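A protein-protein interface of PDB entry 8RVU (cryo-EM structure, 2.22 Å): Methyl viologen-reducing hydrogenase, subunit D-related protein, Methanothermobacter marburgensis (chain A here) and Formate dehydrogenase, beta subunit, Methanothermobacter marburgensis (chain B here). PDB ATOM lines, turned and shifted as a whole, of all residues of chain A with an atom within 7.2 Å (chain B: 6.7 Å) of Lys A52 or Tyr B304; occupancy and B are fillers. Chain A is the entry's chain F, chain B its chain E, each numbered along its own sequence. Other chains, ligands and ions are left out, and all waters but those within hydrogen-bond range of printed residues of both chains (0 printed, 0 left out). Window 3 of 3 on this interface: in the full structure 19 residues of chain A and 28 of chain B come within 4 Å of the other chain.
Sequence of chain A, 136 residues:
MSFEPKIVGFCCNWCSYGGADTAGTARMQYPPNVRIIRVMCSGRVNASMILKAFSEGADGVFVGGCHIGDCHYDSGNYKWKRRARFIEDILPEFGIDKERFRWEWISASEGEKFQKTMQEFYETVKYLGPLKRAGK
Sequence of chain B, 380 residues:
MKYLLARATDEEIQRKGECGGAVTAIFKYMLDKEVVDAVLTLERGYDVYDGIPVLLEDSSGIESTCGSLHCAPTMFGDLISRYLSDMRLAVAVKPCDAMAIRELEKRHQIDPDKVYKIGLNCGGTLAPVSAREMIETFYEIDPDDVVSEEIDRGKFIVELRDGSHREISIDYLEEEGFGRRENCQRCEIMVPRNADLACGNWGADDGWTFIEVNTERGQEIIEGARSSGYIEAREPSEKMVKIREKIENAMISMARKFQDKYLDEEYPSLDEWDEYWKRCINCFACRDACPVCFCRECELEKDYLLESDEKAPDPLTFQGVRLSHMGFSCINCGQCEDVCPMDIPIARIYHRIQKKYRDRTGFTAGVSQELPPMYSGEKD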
ATOM      1  N   ALA A  47     -18.985  -7.341  19.426  1.00  0.00           N
ATOM      2  CA  ALA A  47     -19.750  -8.524  19.809  1.00  0.00           C
ATOM      3  C   ALA A  47     -19.078  -9.813  19.360  1.00  0.00           C
ATOM      4  O   ALA A  47     -19.320 -10.872  19.950  1.00  0.00           O
ATOM      5  CB  ALA A  47     -21.153  -8.445  19.223  1.00  0.00           C
ATOM      6  N   SER A  48     -18.249  -9.754  18.316  1.00  0.00           N
ATOM      7  CA  SER A  48     -17.597 -10.968  17.839  1.00  0.00           C
ATOM      8  C   SER A  48     -16.713 -11.571  18.920  1.00  0.00           C
ATOM      9  O   SER A  48     -16.683 -12.793  19.095  1.00  0.00           O
ATOM     10  CB  SER A  48     -16.780 -10.673  16.581  1.00  0.00           C
ATOM     11  OG  SER A  48     -17.625 -10.482  15.462  1.00  0.00           O
ATOM     12  N   MET A  49     -15.994 -10.729  19.666  1.00  0.00           N
ATOM     13  CA  MET A  49     -15.149 -11.233  20.744  1.00  0.00           C
ATOM     14  C   MET A  49     -15.977 -11.897  21.838  1.00  0.00           C
ATOM     15  O   MET A  49     -15.613 -12.967  22.335  1.00  0.00           O
ATOM     16  CB  MET A  49     -14.312 -10.093  21.323  1.00  0.00           C
ATOM     17  CG  MET A  49     -13.362  -9.455  20.323  1.00  0.00           C
ATOM     18  SD  MET A  49     -12.886  -7.779  20.775  1.00  0.00           S
ATOM     19  CE  MET A  49     -12.210  -7.199  19.224  1.00  0.00           C
ATOM     20  N   ILE A  50     -17.099 -11.281  22.221  1.00  0.00           N
ATOM     21  CA  ILE A  50     -17.939 -11.850  23.275  1.00  0.00           C
ATOM     22  C   ILE A  50     -18.504 -13.193  22.830  1.00  0.00           C
ATOM     23  O   ILE A  50     -18.502 -14.177  23.582  1.00  0.00           O
ATOM     24  CB  ILE A  50     -19.067 -10.870  23.654  1.00  0.00           C
ATOM     25  CG1 ILE A  50     -18.537  -9.439  23.814  1.00  0.00           C
ATOM     26  CG2 ILE A  50     -19.757 -11.320  24.934  1.00  0.00           C
ATOM     27  CD1 ILE A  50     -17.395  -9.296  24.793  1.00  0.00           C
ATOM     28  N   LEU A  51     -19.006 -13.248  21.594  1.00  0.00           N
ATOM     29  CA  LEU A  51     -19.589 -14.483  21.085  1.00  0.00           C
ATOM     30  C   LEU A  51     -18.533 -15.570  20.944  1.00  0.00           C
ATOM     31  O   LEU A  51     -18.800 -16.740  21.233  1.00  0.00           O
ATOM     32  CB  LEU A  51     -20.282 -14.219  19.749  1.00  0.00           C
ATOM     33  CG  LEU A  51     -21.553 -13.372  19.854  1.00  0.00           C
ATOM     34  CD1 LEU A  51     -21.884 -12.727  18.520  1.00  0.00           C
ATOM     35  CD2 LEU A  51     -22.722 -14.204  20.352  1.00  0.00           C
ATOM     36  N   LYS A  52     -17.326 -15.203  20.507  1.00  0.00           N
ATOM     37  CA  LYS A  52     -16.241 -16.173  20.424  1.00  0.00           C
ATOM     38  C   LYS A  52     -15.882 -16.699  21.807  1.00  0.00           C
ATOM     39  O   LYS A  52     -15.651 -17.901  21.982  1.00  0.00           O
ATOM     40  CB  LYS A  52     -15.027 -15.526  19.753  1.00  0.00           C
ATOM     41  CG  LYS A  52     -13.751 -16.365  19.738  1.00  0.00           C
ATOM     42  CD  LYS A  52     -13.797 -17.435  18.660  1.00  0.00           C
ATOM     43  CE  LYS A  52     -12.400 -17.899  18.282  1.00  0.00           C
ATOM     44  NZ  LYS A  52     -12.411 -19.204  17.567  1.00  0.00           N
ATOM     45  N   ALA A  53     -15.834 -15.813  22.804  1.00  0.00           N
ATOM     46  CA  ALA A  53     -15.537 -16.247  24.164  1.00  0.00           C
ATOM     47  C   ALA A  53     -16.580 -17.242  24.656  1.00  0.00           C
ATOM     48  O   ALA A  53     -16.240 -18.293  25.209  1.00  0.00           O
ATOM     49  CB  ALA A  53     -15.464 -15.036  25.095  1.00  0.00           C
ATOM     50  N   PHE A  54     -17.861 -16.929  24.455  1.00  0.00           N
ATOM     51  CA  PHE A  54     -18.909 -17.842  24.905  1.00  0.00           C
ATOM     52  C   PHE A  54     -18.889 -19.156  24.130  1.00  0.00           C
ATOM     53  O   PHE A  54     -19.159 -20.215  24.707  1.00  0.00           O
ATOM     54  CB  PHE A  54     -20.280 -17.174  24.793  1.00  0.00           C
ATOM     55  CG  PHE A  54     -20.632 -16.308  25.976  1.00  0.00           C
ATOM     56  CD1 PHE A  54     -20.583 -16.817  27.266  1.00  0.00           C
ATOM     57  CD2 PHE A  54     -21.014 -14.990  25.798  1.00  0.00           C
ATOM     58  CE1 PHE A  54     -20.903 -16.028  28.350  1.00  0.00           C
ATOM     59  CE2 PHE A  54     -21.338 -14.198  26.884  1.00  0.00           C
ATOM     60  CZ  PHE A  54     -21.281 -14.719  28.159  1.00  0.00           C
ATOM     61  N   SER A  55     -18.570 -19.115  22.835  1.00  0.00           N
ATOM     62  CA  SER A  55     -18.531 -20.339  22.042  1.00  0.00           C
ATOM     63  C   SER A  55     -17.333 -21.209  22.402  1.00  0.00           C
ATOM     64  O   SER A  55     -17.400 -22.437  22.271  1.00  0.00           O
ATOM     65  CB  SER A  55     -18.501 -19.993  20.554  1.00  0.00           C
ATOM     66  OG  SER A  55     -18.336 -21.155  19.762  1.00  0.00           O
ATOM     67  N   GLU A  56     -16.236 -20.600  22.851  1.00  0.00           N
ATOM     68  CA  GLU A  56     -15.027 -21.346  23.174  1.00  0.00           C
ATOM     69  C   GLU A  56     -15.081 -22.009  24.543  1.00  0.00           C
ATOM     70  O   GLU A  56     -14.229 -22.856  24.832  1.00  0.00           O
ATOM     71  CB  GLU A  56     -13.808 -20.418  23.108  1.00  0.00           C
ATOM     72  CG  GLU A  56     -13.342 -20.066  21.697  1.00  0.00           C
ATOM     73  CD  GLU A  56     -13.201 -21.276  20.793  1.00  0.00           C
ATOM     74  OE1 GLU A  56     -12.171 -21.976  20.889  1.00  0.00           O
ATOM     75  OE2 GLU A  56     -14.119 -21.525  19.985  1.00  0.00           O
ATOM     76  N   GLY A  57     -16.047 -21.652  25.387  1.00  0.00           N
ATOM     77  CA  GLY A  57     -16.216 -22.323  26.662  1.00  0.00           C
ATOM     78  C   GLY A  57     -16.357 -21.390  27.847  1.00  0.00           C
ATOM     79  O   GLY A  57     -16.451 -21.849  28.989  1.00  0.00           O
ATOM     80  N   ALA A  58     -16.374 -20.085  27.599  1.00  0.00           N
ATOM     81  CA  ALA A  58     -16.500 -19.126  28.686  1.00  0.00           C
ATOM     82  C   ALA A  58     -17.887 -19.204  29.310  1.00  0.00           C
ATOM     83  O   ALA A  58     -18.897 -19.316  28.610  1.00  0.00           O
ATOM     84  CB  ALA A  58     -16.233 -17.709  28.182  1.00  0.00           C
ATOM     85  N   VAL A  61     -18.419 -13.263  30.708  1.00  0.00           N
ATOM     86  CA  VAL A  61     -17.586 -12.311  29.985  1.00  0.00           C
ATOM     87  C   VAL A  61     -17.744 -10.947  30.640  1.00  0.00           C
ATOM     88  O   VAL A  61     -18.865 -10.431  30.747  1.00  0.00           O
ATOM     89  CB  VAL A  61     -17.947 -12.240  28.491  1.00  0.00           C
ATOM     90  CG1 VAL A  61     -17.079 -11.211  27.786  1.00  0.00           C
ATOM     91  CG2 VAL A  61     -17.796 -13.608  27.840  1.00  0.00           C
ATOM     92  N   GLU B 299     -16.836 -11.801   7.227  1.00  0.00           N
ATOM     93  CA  GLU B 299     -16.144 -12.230   8.438  1.00  0.00           C
ATOM     94  C   GLU B 299     -16.498 -13.662   8.809  1.00  0.00           C
ATOM     95  O   GLU B 299     -15.678 -14.370   9.405  1.00  0.00           O
ATOM     96  CB  GLU B 299     -16.486 -11.287   9.592  1.00  0.00           C
ATOM     97  CG  GLU B 299     -15.763 -11.597  10.890  1.00  0.00           C
ATOM     98  CD  GLU B 299     -16.096 -10.609  11.990  1.00  0.00           C
ATOM     99  OE1 GLU B 299     -16.923  -9.705  11.747  1.00  0.00           O
ATOM    100  OE2 GLU B 299     -15.538 -10.739  13.098  1.00  0.00           O
ATOM    101  N   GLU B 301     -16.527 -16.204   7.154  1.00  0.00           N
ATOM    102  CA  GLU B 301     -15.669 -17.166   6.477  1.00  0.00           C
ATOM    103  C   GLU B 301     -14.233 -17.150   6.986  1.00  0.00           C
ATOM    104  O   GLU B 301     -13.408 -17.920   6.486  1.00  0.00           O
ATOM    105  CB  GLU B 301     -15.679 -16.905   4.968  1.00  0.00           C
ATOM    106  CG  GLU B 301     -17.034 -16.490   4.429  1.00  0.00           C
ATOM    107  CD  GLU B 301     -17.250 -16.930   2.995  1.00  0.00           C
ATOM    108  OE1 GLU B 301     -17.081 -18.134   2.711  1.00  0.00           O
ATOM    109  OE2 GLU B 301     -17.589 -16.073   2.155  1.00  0.00           O
ATOM    110  N   LYS B 302     -13.914 -16.303   7.961  1.00  0.00           N
ATOM    111  CA  LYS B 302     -12.577 -16.295   8.530  1.00  0.00           C
ATOM    112  C   LYS B 302     -12.306 -17.600   9.275  1.00  0.00           C
ATOM    113  O   LYS B 302     -13.220 -18.309   9.703  1.00  0.00           O
ATOM    114  CB  LYS B 302     -12.400 -15.106   9.474  1.00  0.00           C
ATOM    115  CG  LYS B 302     -12.581 -13.748   8.813  1.00  0.00           C
ATOM    116  CD  LYS B 302     -11.292 -13.271   8.161  1.00  0.00           C
ATOM    117  CE  LYS B 302     -11.320 -11.778   7.883  1.00  0.00           C
ATOM    118  NZ  LYS B 302     -12.617 -11.323   7.312  1.00  0.00           N
ATOM    119  N   ASP B 303     -11.017 -17.915   9.424  1.00  0.00           N
ATOM    120  CA  ASP B 303     -10.633 -19.172  10.062  1.00  0.00           C
ATOM    121  C   ASP B 303     -11.140 -19.244  11.498  1.00  0.00           C
ATOM    122  O   ASP B 303     -11.635 -20.288  11.936  1.00  0.00           O
ATOM    123  CB  ASP B 303      -9.113 -19.346  10.031  1.00  0.00           C
ATOM    124  CG  ASP B 303      -8.367 -18.054  10.304  1.00  0.00           C
ATOM    125  OD1 ASP B 303      -8.332 -17.185   9.407  1.00  0.00           O
ATOM    126  OD2 ASP B 303      -7.819 -17.906  11.416  1.00  0.00           O
ATOM    127  N   TYR B 304     -11.019 -18.148  12.250  1.00  0.00           N
ATOM    128  CA  TYR B 304     -11.410 -18.169  13.654  1.00  0.00           C
ATOM    129  C   TYR B 304     -12.921 -18.207  13.849  1.00  0.00           C
ATOM    130  O   TYR B 304     -13.373 -18.405  14.982  1.00  0.00           O
ATOM    131  CB  TYR B 304     -10.821 -16.964  14.394  1.00  0.00           C
ATOM    132  CG  TYR B 304     -11.075 -15.623  13.742  1.00  0.00           C
ATOM    133  CD1 TYR B 304     -12.258 -14.931  13.967  1.00  0.00           C
ATOM    134  CD2 TYR B 304     -10.125 -15.044  12.911  1.00  0.00           C
ATOM    135  CE1 TYR B 304     -12.490 -13.705  13.377  1.00  0.00           C
ATOM    136  CE2 TYR B 304     -10.350 -13.819  12.316  1.00  0.00           C
ATOM    137  CZ  TYR B 304     -11.533 -13.154  12.552  1.00  0.00           C
ATOM    138  OH  TYR B 304     -11.760 -11.933  11.965  1.00  0.00           O
ATOM    139  N   LEU B 305     -13.706 -18.026  12.789  1.00  0.00           N
ATOM    140  CA  LEU B 305     -15.158 -18.165  12.847  1.00  0.00           C
ATOM    141  C   LEU B 305     -15.685 -19.312  12.002  1.00  0.00           C
ATOM    142  O   LEU B 305     -16.560 -20.052  12.457  1.00  0.00           O
ATOM    143  CB  LEU B 305     -15.838 -16.869  12.388  1.00  0.00           C
ATOM    144  CG  LEU B 305     -15.858 -15.666  13.333  1.00  0.00           C
ATOM    145  CD1 LEU B 305     -16.806 -14.612  12.787  1.00  0.00           C
ATOM    146  CD2 LEU B 305     -16.262 -16.060  14.745  1.00  0.00           C
ATOM    147  N   LEU B 306     -15.175 -19.477  10.784  1.00  0.00           N
ATOM    148  CA  LEU B 306     -15.719 -20.474   9.874  1.00  0.00           C
ATOM    149  C   LEU B 306     -15.589 -21.872  10.464  1.00  0.00           C
ATOM    150  O   LEU B 306     -14.542 -22.249  10.997  1.00  0.00           O
ATOM    151  CB  LEU B 306     -15.001 -20.408   8.525  1.00  0.00           C
ATOM    152  CG  LEU B 306     -15.441 -21.418   7.461  1.00  0.00           C
ATOM    153  CD1 LEU B 306     -16.828 -21.078   6.943  1.00  0.00           C
ATOM    154  CD2 LEU B 306     -14.441 -21.466   6.318  1.00  0.00           C
ATOM    155  N   LEU B 316     -23.816 -19.668  17.510  1.00  0.00           N
ATOM    156  CA  LEU B 316     -23.229 -18.434  18.010  1.00  0.00           C
ATOM    157  C   LEU B 316     -22.346 -17.806  16.939  1.00  0.00           C
ATOM    158  O   LEU B 316     -22.737 -16.810  16.326  1.00  0.00           O
ATOM    159  CB  LEU B 316     -22.421 -18.692  19.284  1.00  0.00           C
ATOM    160  CG  LEU B 316     -23.229 -18.804  20.579  1.00  0.00           C
ATOM    161  CD1 LEU B 316     -22.359 -19.350  21.700  1.00  0.00           C
ATOM    162  CD2 LEU B 316     -23.820 -17.459  20.970  1.00  0.00           C
ATOM    163  N   THR B 317     -21.217 -18.444  16.627  1.00  0.00           N
ATOM    164  CA  THR B 317     -20.199 -17.837  15.777  1.00  0.00           C
ATOM    165  C   THR B 317     -20.652 -17.630  14.336  1.00  0.00           C
ATOM    166  O   THR B 317     -19.861 -17.119  13.536  1.00  0.00           O
ATOM    167  CB  THR B 317     -18.932 -18.695  15.795  1.00  0.00           C
ATOM    168  OG1 THR B 317     -19.288 -20.082  15.743  1.00  0.00           O
ATOM    169  CG2 THR B 317     -18.121 -18.428  17.054  1.00  0.00           C
ATOM    170  N   VAL B 321     -22.954 -13.713  15.179  1.00  0.00           N
ATOM    171  CA  VAL B 321     -22.022 -12.786  14.547  1.00  0.00           C
ATOM    172  C   VAL B 321     -22.728 -11.977  13.466  1.00  0.00           C
ATOM    173  O   VAL B 321     -22.600 -10.748  13.407  1.00  0.00           O
ATOM    174  CB  VAL B 321     -20.803 -13.542  13.988  1.00  0.00           C
ATOM    175  CG1 VAL B 321     -19.915 -12.597  13.186  1.00  0.00           C
ATOM    176  CG2 VAL B 321     -20.017 -14.177  15.119  1.00  0.00           C
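The backbone carbonyl oxygen (O) of Tyr B304 sits at hydrogen-bond distance from the side-chain amino group (NZ) of Lys A52, at 2.9 Å. The side-chain carboxylate (OE2) of Glu B299 is in hydrogen-bond range of the side-chain hydroxyl (OG) of Ser A48 (3.2 Å).
The side-chain amino group (NZ) of Lys A52 lies within salt-bridge range of the side-chain carboxylate (OE2) of Glu A56. The backbone NH (N) of Val B321 is in hydrogen-bond range of the backbone carbonyl oxygen (O) of Leu B316 (3.3 Å).
Of the 13 printed residues of chain A, 4 touch a printed residue of chain B. Hydrophobic or aromatic side chains of chain A that line the printed part of chain B: Leu A51. Along chain B the printed residues that touch a printed residue of chain A span positions 299 to 321.
Among the printed residues, merely in contact across the chains: Ser A48 with Val B321 (3.9 Å), Leu A51 with Leu B316 (3.5 Å), Leu A51 with Val B321 (3.6 Å), Ser A55 with Leu B316 (3.96 Å) and Ser A55 with Thr B317 (3.8 Å).
Of chain B, only Tyr B304 comes within 4 Å of Lys A52. Tyr B304 touches just one residue of chain A: Lys A52. Of the printed residues of chain B, Ser A48 touches Glu B299 and Val B321. Of the printed residues of chain B, Leu A51 touches Leu B316 (3.5 Å) and Val B321 (3.6 Å). Of the printed residues of chain A, Thr B317 touches Ser A55 (3.8 Å). Printed residues of chain B within 4 Å of Ser A55: Leu B316 and Thr B317. Of the printed residues of chain A, Leu B316 touches Leu A51 and Ser A55. Ile A50 touches none of the printed residues of chain B. Ala A47 touches none of the printed residues of chain B. The nearest residue of chain B that does not touch Lys A52 is Thr B317 (4.5 Å). The nearest residue of chain A that does not touch Tyr B304 is Glu A56 (5.9 Å). The nearest printed residue of chain B that does not touch Leu A51 is Thr B317 (4.6 Å).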
